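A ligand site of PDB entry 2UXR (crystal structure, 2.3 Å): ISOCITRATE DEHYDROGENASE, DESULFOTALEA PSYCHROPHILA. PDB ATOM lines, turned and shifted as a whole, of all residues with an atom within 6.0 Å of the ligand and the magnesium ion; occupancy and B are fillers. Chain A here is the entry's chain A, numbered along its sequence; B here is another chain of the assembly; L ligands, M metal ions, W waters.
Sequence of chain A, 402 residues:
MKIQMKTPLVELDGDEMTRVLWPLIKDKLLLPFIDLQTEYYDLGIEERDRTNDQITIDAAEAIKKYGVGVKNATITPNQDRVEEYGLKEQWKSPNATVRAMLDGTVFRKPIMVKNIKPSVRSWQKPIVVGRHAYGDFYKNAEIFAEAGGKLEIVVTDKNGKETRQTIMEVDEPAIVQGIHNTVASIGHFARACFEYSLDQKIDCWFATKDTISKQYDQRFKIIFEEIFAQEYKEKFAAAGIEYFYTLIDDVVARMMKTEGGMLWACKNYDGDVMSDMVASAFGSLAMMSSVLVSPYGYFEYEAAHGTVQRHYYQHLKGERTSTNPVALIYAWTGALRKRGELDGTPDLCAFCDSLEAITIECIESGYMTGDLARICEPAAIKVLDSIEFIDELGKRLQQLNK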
ATOM      1  N   THR A  74     -23.001  25.377 -33.385  1.00  0.00           N
ATOM      2  CA  THR A  74     -24.128  24.993 -34.245  1.00  0.00           C
ATOM      3  C   THR A  74     -25.352  24.738 -33.438  1.00  0.00           C
ATOM      4  O   THR A  74     -25.242  24.406 -32.274  1.00  0.00           O
ATOM      5  CB  THR A  74     -23.801  23.725 -35.035  1.00  0.00           C
ATOM      6  OG1 THR A  74     -23.150  22.772 -34.188  1.00  0.00           O
ATOM      7  CG2 THR A  74     -22.899  24.035 -36.206  1.00  0.00           C
ATOM      8  N   ILE A  75     -26.530  24.880 -34.042  1.00  0.00           N
ATOM      9  CA  ILE A  75     -27.780  24.415 -33.481  1.00  0.00           C
ATOM     10  C   ILE A  75     -27.936  22.922 -33.773  1.00  0.00           C
ATOM     11  O   ILE A  75     -27.777  22.482 -34.916  1.00  0.00           O
ATOM     12  CB  ILE A  75     -29.011  25.161 -34.155  1.00  0.00           C
ATOM     13  CG1 ILE A  75     -29.087  26.632 -33.739  1.00  0.00           C
ATOM     14  CG2 ILE A  75     -30.343  24.455 -33.891  1.00  0.00           C
ATOM     15  CD1 ILE A  75     -29.823  27.495 -34.795  1.00  0.00           C
ATOM     16  N   THR A  76     -28.265  22.140 -32.745  1.00  0.00           N
ATOM     17  CA  THR A  76     -28.847  20.814 -32.957  1.00  0.00           C
ATOM     18  C   THR A  76     -30.372  20.951 -32.825  1.00  0.00           C
ATOM     19  O   THR A  76     -30.871  21.316 -31.753  1.00  0.00           O
ATOM     20  CB  THR A  76     -28.288  19.786 -31.987  1.00  0.00           C
ATOM     21  OG1 THR A  76     -26.872  19.788 -32.120  1.00  0.00           O
ATOM     22  CG2 THR A  76     -28.865  18.417 -32.265  1.00  0.00           C
ATOM     23  N   SER A  93     -27.095  16.077 -34.413  1.00  0.00           N
ATOM     24  CA  SER A  93     -25.970  16.915 -33.983  1.00  0.00           C
ATOM     25  C   SER A  93     -24.741  16.890 -34.903  1.00  0.00           C
ATOM     26  O   SER A  93     -24.127  15.855 -35.079  1.00  0.00           O
ATOM     27  CB  SER A  93     -25.529  16.567 -32.550  1.00  0.00           C
ATOM     28  OG  SER A  93     -24.291  17.220 -32.313  1.00  0.00           O
ATOM     29  N   PRO A  94     -24.384  18.044 -35.490  1.00  0.00           N
ATOM     30  CA  PRO A  94     -23.175  18.018 -36.343  1.00  0.00           C
ATOM     31  C   PRO A  94     -21.906  17.678 -35.581  1.00  0.00           C
ATOM     32  O   PRO A  94     -20.978  17.150 -36.151  1.00  0.00           O
ATOM     33  CB  PRO A  94     -23.111  19.428 -36.978  1.00  0.00           C
ATOM     34  CG  PRO A  94     -24.049  20.229 -36.275  1.00  0.00           C
ATOM     35  CD  PRO A  94     -25.026  19.371 -35.458  1.00  0.00           C
ATOM     36  N   ASN A  95     -21.886  18.014 -34.292  1.00  0.00           N
ATOM     37  CA  ASN A  95     -20.779  17.657 -33.407  1.00  0.00           C
ATOM     38  C   ASN A  95     -20.696  16.141 -33.255  1.00  0.00           C
ATOM     39  O   ASN A  95     -19.633  15.598 -33.327  1.00  0.00           O
ATOM     40  CB  ASN A  95     -20.945  18.326 -32.017  1.00  0.00           C
ATOM     41  CG  ASN A  95     -20.943  19.825 -32.095  1.00  0.00           C
ATOM     42  OD1 ASN A  95     -21.845  20.521 -31.556  1.00  0.00           O
ATOM     43  ND2 ASN A  95     -19.947  20.354 -32.788  1.00  0.00           N
ATOM     44  N   ALA A  96     -21.813  15.498 -32.942  1.00  0.00           N
ATOM     45  CA  ALA A  96     -21.902  14.062 -32.849  1.00  0.00           C
ATOM     46  C   ALA A  96     -21.404  13.388 -34.148  1.00  0.00           C
ATOM     47  O   ALA A  96     -20.601  12.439 -34.115  1.00  0.00           O
ATOM     48  CB  ALA A  96     -23.342  13.681 -32.576  1.00  0.00           C
ATOM     49  N   ARG A  99     -17.523  14.076 -34.566  1.00  0.00           N
ATOM     50  CA  ARG A  99     -16.709  13.339 -33.563  1.00  0.00           C
ATOM     51  C   ARG A  99     -16.735  11.834 -33.820  1.00  0.00           C
ATOM     52  O   ARG A  99     -15.773  11.133 -33.567  1.00  0.00           O
ATOM     53  CB  ARG A  99     -17.131  13.668 -32.113  1.00  0.00           C
ATOM     54  CG  ARG A  99     -16.943  15.175 -31.686  1.00  0.00           C
ATOM     55  CD  ARG A  99     -17.771  15.472 -30.429  1.00  0.00           C
ATOM     56  NE  ARG A  99     -17.798  16.897 -30.057  1.00  0.00           N
ATOM     57  CZ  ARG A  99     -18.696  17.510 -29.310  1.00  0.00           C
ATOM     58  NH1 ARG A  99     -19.741  16.868 -28.809  1.00  0.00           N
ATOM     59  NH2 ARG A  99     -18.570  18.796 -29.103  1.00  0.00           N
ATOM     60  N   ARG A 108     -10.988  19.975 -22.512  1.00  0.00           N
ATOM     61  CA  ARG A 108     -11.696  21.207 -22.144  1.00  0.00           C
ATOM     62  C   ARG A 108     -11.086  21.780 -20.883  1.00  0.00           C
ATOM     63  O   ARG A 108     -11.090  21.154 -19.812  1.00  0.00           O
ATOM     64  CB  ARG A 108     -13.196  20.958 -22.012  1.00  0.00           C
ATOM     65  CG  ARG A 108     -13.883  20.826 -23.364  1.00  0.00           C
ATOM     66  CD  ARG A 108     -15.344  20.631 -23.330  1.00  0.00           C
ATOM     67  NE  ARG A 108     -15.830  20.580 -24.699  1.00  0.00           N
ATOM     68  CZ  ARG A 108     -17.080  20.406 -25.103  1.00  0.00           C
ATOM     69  NH1 ARG A 108     -18.069  20.233 -24.235  1.00  0.00           N
ATOM     70  NH2 ARG A 108     -17.334  20.392 -26.402  1.00  0.00           N
ATOM     71  N   ARG A 131     -12.938  14.595 -22.195  1.00  0.00           N
ATOM     72  CA  ARG A 131     -14.216  13.994 -22.579  1.00  0.00           C
ATOM     73  C   ARG A 131     -14.114  13.029 -23.767  1.00  0.00           C
ATOM     74  O   ARG A 131     -13.703  13.417 -24.892  1.00  0.00           O
ATOM     75  CB  ARG A 131     -15.240  15.087 -22.866  1.00  0.00           C
ATOM     76  CG  ARG A 131     -16.471  14.651 -23.646  1.00  0.00           C
ATOM     77  CD  ARG A 131     -17.226  15.881 -24.117  1.00  0.00           C
ATOM     78  NE  ARG A 131     -18.461  15.458 -24.734  1.00  0.00           N
ATOM     79  CZ  ARG A 131     -19.378  16.255 -25.265  1.00  0.00           C
ATOM     80  NH1 ARG A 131     -19.166  17.581 -25.308  1.00  0.00           N
ATOM     81  NH2 ARG A 131     -20.513  15.727 -25.720  1.00  0.00           N
ATOM     82  N   TYR A 138     -24.710   9.787 -27.849  1.00  0.00           N
ATOM     83  CA  TYR A 138     -24.492  10.496 -29.108  1.00  0.00           C
ATOM     84  C   TYR A 138     -24.496   9.629 -30.437  1.00  0.00           C
ATOM     85  O   TYR A 138     -24.182  10.157 -31.492  1.00  0.00           O
ATOM     86  CB  TYR A 138     -23.176  11.278 -29.040  1.00  0.00           C
ATOM     87  CG  TYR A 138     -23.237  12.464 -28.126  1.00  0.00           C
ATOM     88  CD1 TYR A 138     -23.601  13.710 -28.628  1.00  0.00           C
ATOM     89  CD2 TYR A 138     -22.963  12.339 -26.744  1.00  0.00           C
ATOM     90  CE1 TYR A 138     -23.675  14.829 -27.773  1.00  0.00           C
ATOM     91  CE2 TYR A 138     -23.025  13.447 -25.884  1.00  0.00           C
ATOM     92  CZ  TYR A 138     -23.381  14.680 -26.412  1.00  0.00           C
ATOM     93  OH  TYR A 138     -23.436  15.769 -25.591  1.00  0.00           O
ATOM     94  N   ASN A 268     -18.493  10.400 -22.578  1.00  0.00           N
ATOM     95  CA  ASN A 268     -19.046  11.389 -23.487  1.00  0.00           C
ATOM     96  C   ASN A 268     -20.104  12.286 -22.817  1.00  0.00           C
ATOM     97  O   ASN A 268     -19.979  13.511 -22.787  1.00  0.00           O
ATOM     98  CB  ASN A 268     -19.601  10.686 -24.754  1.00  0.00           C
ATOM     99  CG  ASN A 268     -19.738  11.642 -25.946  1.00  0.00           C
ATOM    100  OD1 ASN A 268     -19.529  12.854 -25.787  1.00  0.00           O
ATOM    101  ND2 ASN A 268     -20.032  11.090 -27.137  1.00  0.00           N
ATOM    102  N   ASP A 272     -19.779  16.377 -21.241  1.00  0.00           N
ATOM    103  CA  ASP A 272     -20.604  17.499 -21.718  1.00  0.00           C
ATOM    104  C   ASP A 272     -21.096  18.321 -20.526  1.00  0.00           C
ATOM    105  O   ASP A 272     -21.004  19.528 -20.515  1.00  0.00           O
ATOM    106  CB  ASP A 272     -21.780  16.976 -22.545  1.00  0.00           C
ATOM    107  CG  ASP A 272     -22.666  18.068 -23.039  1.00  0.00           C
ATOM    108  OD1 ASP A 272     -22.130  19.015 -23.627  1.00  0.00           O
ATOM    109  OD2 ASP A 272     -23.904  18.045 -22.831  1.00  0.00           O
ATOM    110  N   VAL A 273     -21.644  17.626 -19.525  1.00  0.00           N
ATOM    111  CA  VAL A 273     -22.220  18.226 -18.316  1.00  0.00           C
ATOM    112  C   VAL A 273     -21.137  18.933 -17.492  1.00  0.00           C
ATOM    113  O   VAL A 273     -21.233  20.135 -17.266  1.00  0.00           O
ATOM    114  CB  VAL A 273     -22.962  17.111 -17.492  1.00  0.00           C
ATOM    115  CG1 VAL A 273     -23.567  17.645 -16.138  1.00  0.00           C
ATOM    116  CG2 VAL A 273     -24.036  16.542 -18.353  1.00  0.00           C
ATOM    117  N   SER A 275     -17.941  19.609 -18.168  1.00  0.00           N
ATOM    118  CA  SER A 275     -17.183  20.677 -18.797  1.00  0.00           C
ATOM    119  C   SER A 275     -17.878  22.041 -18.690  1.00  0.00           C
ATOM    120  O   SER A 275     -17.200  23.069 -18.541  1.00  0.00           O
ATOM    121  CB  SER A 275     -16.759  20.355 -20.235  1.00  0.00           C
ATOM    122  OG  SER A 275     -17.820  20.519 -21.163  1.00  0.00           O
ATOM    123  N   ASP A 276     -19.212  22.043 -18.794  1.00  0.00           N
ATOM    124  CA  ASP A 276     -19.980  23.306 -18.575  1.00  0.00           C
ATOM    125  C   ASP A 276     -19.961  23.777 -17.077  1.00  0.00           C
ATOM    126  O   ASP A 276     -19.773  24.959 -16.754  1.00  0.00           O
ATOM    127  CB  ASP A 276     -21.425  23.152 -19.094  1.00  0.00           C
ATOM    128  CG  ASP A 276     -21.593  23.604 -20.530  1.00  0.00           C
ATOM    129  OD1 ASP A 276     -20.616  23.817 -21.257  1.00  0.00           O
ATOM    130  OD2 ASP A 276     -22.754  23.766 -20.951  1.00  0.00           O
ATOM    131  N   GLU A 302     -12.767  23.896 -31.254  1.00  0.00           N
ATOM    132  CA  GLU A 302     -14.113  24.399 -31.254  1.00  0.00           C
ATOM    133  C   GLU A 302     -14.361  25.272 -29.969  1.00  0.00           C
ATOM    134  O   GLU A 302     -13.551  25.272 -29.018  1.00  0.00           O
ATOM    135  CB  GLU A 302     -15.043  23.171 -31.284  1.00  0.00           C
ATOM    136  CG  GLU A 302     -15.099  22.546 -29.916  1.00  0.00           C
ATOM    137  CD  GLU A 302     -15.865  21.279 -29.777  1.00  0.00           C
ATOM    138  OE1 GLU A 302     -16.790  20.978 -30.590  1.00  0.00           O
ATOM    139  OE2 GLU A 302     -15.549  20.605 -28.784  1.00  0.00           O
ATOM    140  N   ALA A 303     -15.456  26.024 -29.937  1.00  0.00           N
ATOM    141  CA  ALA A 303     -15.979  26.534 -28.659  1.00  0.00           C
ATOM    142  C   ALA A 303     -16.819  25.413 -27.944  1.00  0.00           C
ATOM    143  O   ALA A 303     -17.403  24.581 -28.618  1.00  0.00           O
ATOM    144  CB  ALA A 303     -16.795  27.718 -28.919  1.00  0.00           C
ATOM    145  N   ALA A 304     -16.855  25.325 -26.617  1.00  0.00           N
ATOM    146  CA  ALA A 304     -17.675  24.262 -25.985  1.00  0.00           C
ATOM    147  C   ALA A 304     -19.142  24.705 -25.777  1.00  0.00           C
ATOM    148  O   ALA A 304     -20.069  23.882 -25.553  1.00  0.00           O
ATOM    149  CB  ALA A 304     -17.049  23.835 -24.665  1.00  0.00           C
ATOM    150  N   HIS A 305     -19.347  26.012 -25.891  1.00  0.00           N
ATOM    151  CA  HIS A 305     -20.578  26.613 -25.494  1.00  0.00           C
ATOM    152  C   HIS A 305     -21.542  26.566 -26.671  1.00  0.00           C
ATOM    153  O   HIS A 305     -21.226  25.947 -27.674  1.00  0.00           O
ATOM    154  CB  HIS A 305     -20.308  27.984 -24.910  1.00  0.00           C
ATOM    155  CG  HIS A 305     -19.694  28.979 -25.849  1.00  0.00           C
ATOM    156  ND1 HIS A 305     -20.352  29.482 -26.940  1.00  0.00           N
ATOM    157  CD2 HIS A 305     -18.508  29.650 -25.787  1.00  0.00           C
ATOM    158  CE1 HIS A 305     -19.600  30.384 -27.540  1.00  0.00           C
ATOM    159  NE2 HIS A 305     -18.471  30.509 -26.861  1.00  0.00           N
ATOM    160  N   LYS B 209     -31.166  16.206 -22.218  1.00  0.00           N
ATOM    161  CA  LYS B 209     -30.437  16.513 -23.451  1.00  0.00           C
ATOM    162  C   LYS B 209     -31.265  16.112 -24.672  1.00  0.00           C
ATOM    163  O   LYS B 209     -30.879  15.221 -25.450  1.00  0.00           O
ATOM    164  CB  LYS B 209     -29.079  15.839 -23.438  1.00  0.00           C
ATOM    165  CG  LYS B 209     -28.150  16.354 -24.482  1.00  0.00           C
ATOM    166  CD  LYS B 209     -27.433  17.614 -24.052  1.00  0.00           C
ATOM    167  CE  LYS B 209     -26.640  18.190 -25.263  1.00  0.00           C
ATOM    168  NZ  LYS B 209     -25.782  19.235 -24.816  1.00  0.00           N
ATOM    169  N   THR B 211     -32.059  17.392 -27.441  1.00  0.00           N
ATOM    170  CA  THR B 211     -31.556  17.652 -28.780  1.00  0.00           C
ATOM    171  C   THR B 211     -30.749  16.443 -29.341  1.00  0.00           C
ATOM    172  O   THR B 211     -30.684  16.251 -30.564  1.00  0.00           O
ATOM    173  CB  THR B 211     -30.675  18.858 -28.758  1.00  0.00           C
ATOM    174  OG1 THR B 211     -29.672  18.653 -27.777  1.00  0.00           O
ATOM    175  CG2 THR B 211     -31.530  20.178 -28.473  1.00  0.00           C
ATOM    176  N   ILE B 212     -30.160  15.676 -28.429  1.00  0.00           N
ATOM    177  CA  ILE B 212     -29.395  14.464 -28.749  1.00  0.00           C
ATOM    178  C   ILE B 212     -30.305  13.247 -28.705  1.00  0.00           C
ATOM    179  O   ILE B 212     -30.207  12.368 -29.550  1.00  0.00           O
ATOM    180  CB  ILE B 212     -28.167  14.277 -27.809  1.00  0.00           C
ATOM    181  CG1 ILE B 212     -27.233  15.494 -27.953  1.00  0.00           C
ATOM    182  CG2 ILE B 212     -27.384  12.954 -28.101  1.00  0.00           C
ATOM    183  CD1 ILE B 212     -26.871  15.833 -29.411  1.00  0.00           C
ATOM    184  N   ASP B 249     -26.527  20.449 -19.806  1.00  0.00           N
ATOM    185  CA  ASP B 249     -25.201  21.091 -19.653  1.00  0.00           C
ATOM    186  C   ASP B 249     -25.349  22.600 -19.275  1.00  0.00           C
ATOM    187  O   ASP B 249     -24.653  23.126 -18.394  1.00  0.00           O
ATOM    188  CB  ASP B 249     -24.267  20.797 -20.824  1.00  0.00           C
ATOM    189  CG  ASP B 249     -24.838  21.201 -22.194  1.00  0.00           C
ATOM    190  OD1 ASP B 249     -26.060  21.408 -22.399  1.00  0.00           O
ATOM    191  OD2 ASP B 249     -24.021  21.268 -23.132  1.00  0.00           O
HETATM  192  C1  LIG L   1     -20.876  20.776 -26.687  1.00  0.00           C
HETATM  193  O1  LIG L   1     -20.675  20.662 -25.425  1.00  0.00           O
HETATM  194  O2  LIG L   1     -19.908  20.690 -27.498  1.00  0.00           O
HETATM  195  C2  LIG L   1     -22.267  21.015 -27.209  1.00  0.00           C
HETATM  196  O3  LIG L   1     -23.102  21.058 -26.119  1.00  0.00           O
HETATM  197  C3  LIG L   1     -22.806  19.887 -28.072  1.00  0.00           C
HETATM  198  C4  LIG L   1     -24.217  20.328 -28.575  1.00  0.00           C
HETATM  199  C5  LIG L   1     -24.729  19.337 -29.605  1.00  0.00           C
HETATM  200  O4  LIG L   1     -25.966  19.167 -29.746  1.00  0.00           O
HETATM  201  O5  LIG L   1     -23.933  18.670 -30.337  1.00  0.00           O
HETATM  202  C6  LIG L   1     -22.737  18.574 -27.308  1.00  0.00           C
HETATM  203  O6  LIG L   1     -23.807  18.061 -26.861  1.00  0.00           O
HETATM  204  O7  LIG L   1     -21.627  17.989 -27.126  1.00  0.00           O
HETATM  205 MG    MG M   1     -22.083  20.996 -24.010  1.00  0.00          MG
HETATM  206  O   HOH W   1     -27.587  20.247 -28.212  1.00  0.00           O
HETATM  207  O   HOH W   2     -20.524  21.142 -22.499  1.00  0.00           O
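OG of Ser 93 is in hydrogen-bond range of O5 of the ligand (2.5 Å).
The side-chain hydroxyl (OG1) of Thr 76 sits at hydrogen-bond distance from an oxygen (O4) of the ligand, 2.6 Å away.
The side-chain hydroxyl of Tyr 138 lies within hydrogen-bond range of an oxygen (O6) of the ligand, at 2.6 Å.
NH1 of Arg 99 lies within salt-bridge range of O7 of the ligand, at 2.8 Å.
NH2 of Arg 108 is in salt-bridge range of O2 of the ligand, at 2.8 Å.
An oxygen (O7) of the ligand lies within salt-bridge range of the guanidinium group (NH2) of Arg 131, at 2.9 Å.
OD1 of Asn 95 sits close to O5 of the ligand.
O6 of the ligand lies within salt-bridge range of NZ of Lys 209 of chain B (3.1 Å).
The side-chain hydroxyl (OG) of Ser 275 lies within hydrogen-bond range of the backbone carbonyl oxygen (O) of Asp 272 (3.4 Å).
The side-chain carboxylate (OD1) of Asp 249 of chain B lies within salt-bridge range of the side-chain amino group (NZ) of Lys 209 of chain B (3.3 Å).
The backbone NH (N) of Asn 95 sits close to the side-chain hydroxyl (OG) of Ser 93, at 3.2 Å.
The backbone NH of Ala 96 sits at hydrogen-bond distance from the side-chain hydroxyl of Ser 93 (3.1 Å).
OH of Tyr 138 lies within hydrogen-bond range of NH2 of Arg 131 (2.9 Å).
The side-chain carboxylate (OE1) of Glu 302 lies within salt-bridge range of the guanidinium group (NH2) of Arg 99, at 3.2 Å.
NH2 of Arg 108 lies within salt-bridge range of OE2 of Glu 302 (3.0 Å).
The guanidinium group of Arg 131 lies within hydrogen-bond range of the side-chain amide oxygen of Asn 268 (3.0 Å).
The backbone carbonyl oxygen of Ala 304 sits close to an oxygen (O1) of the ligand, at 3.3 Å.
Residues that only touch the ligand: Ile 212 of chain B (3.5 Å).
Within 4 Å of the ligand: Thr 76, Ser 93, Asn 95, Arg 99, Arg 108, Arg 131, Tyr 138, Asp 272, Ala 304, Lys 209 of chain B, Ile 212 of chain B and Asp 249 of chain B.
The nearest printed residue that does not touch the ligand is Thr 211 of chain B (4.2 Å).
Ala 304 touches the magnesium ion (O to MG, 3.8 Å).
Along chain A the residues within 4 Å of the magnesium ion span positions 272 to 304.
The magnesium ion is bound by the side-chain carboxylate of Asp 272 (2.0 Å), an oxygen (O1) of the ligand (2.0 Å), the side-chain carboxylate of Asp 249 of chain B (2.1 Å), water W2 (2.2 Å) and an oxygen (O3) of the ligand (2.3 Å).
Water W2 lies within hydrogen-bond range of the backbone carbonyl oxygen of Asp 272 (2.6 Å), the side-chain carboxylate of Asp 276 (3.0 Å), the side-chain hydroxyl of Ser 275 (3.1 Å) and the guanidinium group of Arg 108 (3.1 Å).
Water W1 bridges an oxygen (O4) of the ligand and the side-chain hydroxyl of Thr 211 of chain B.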
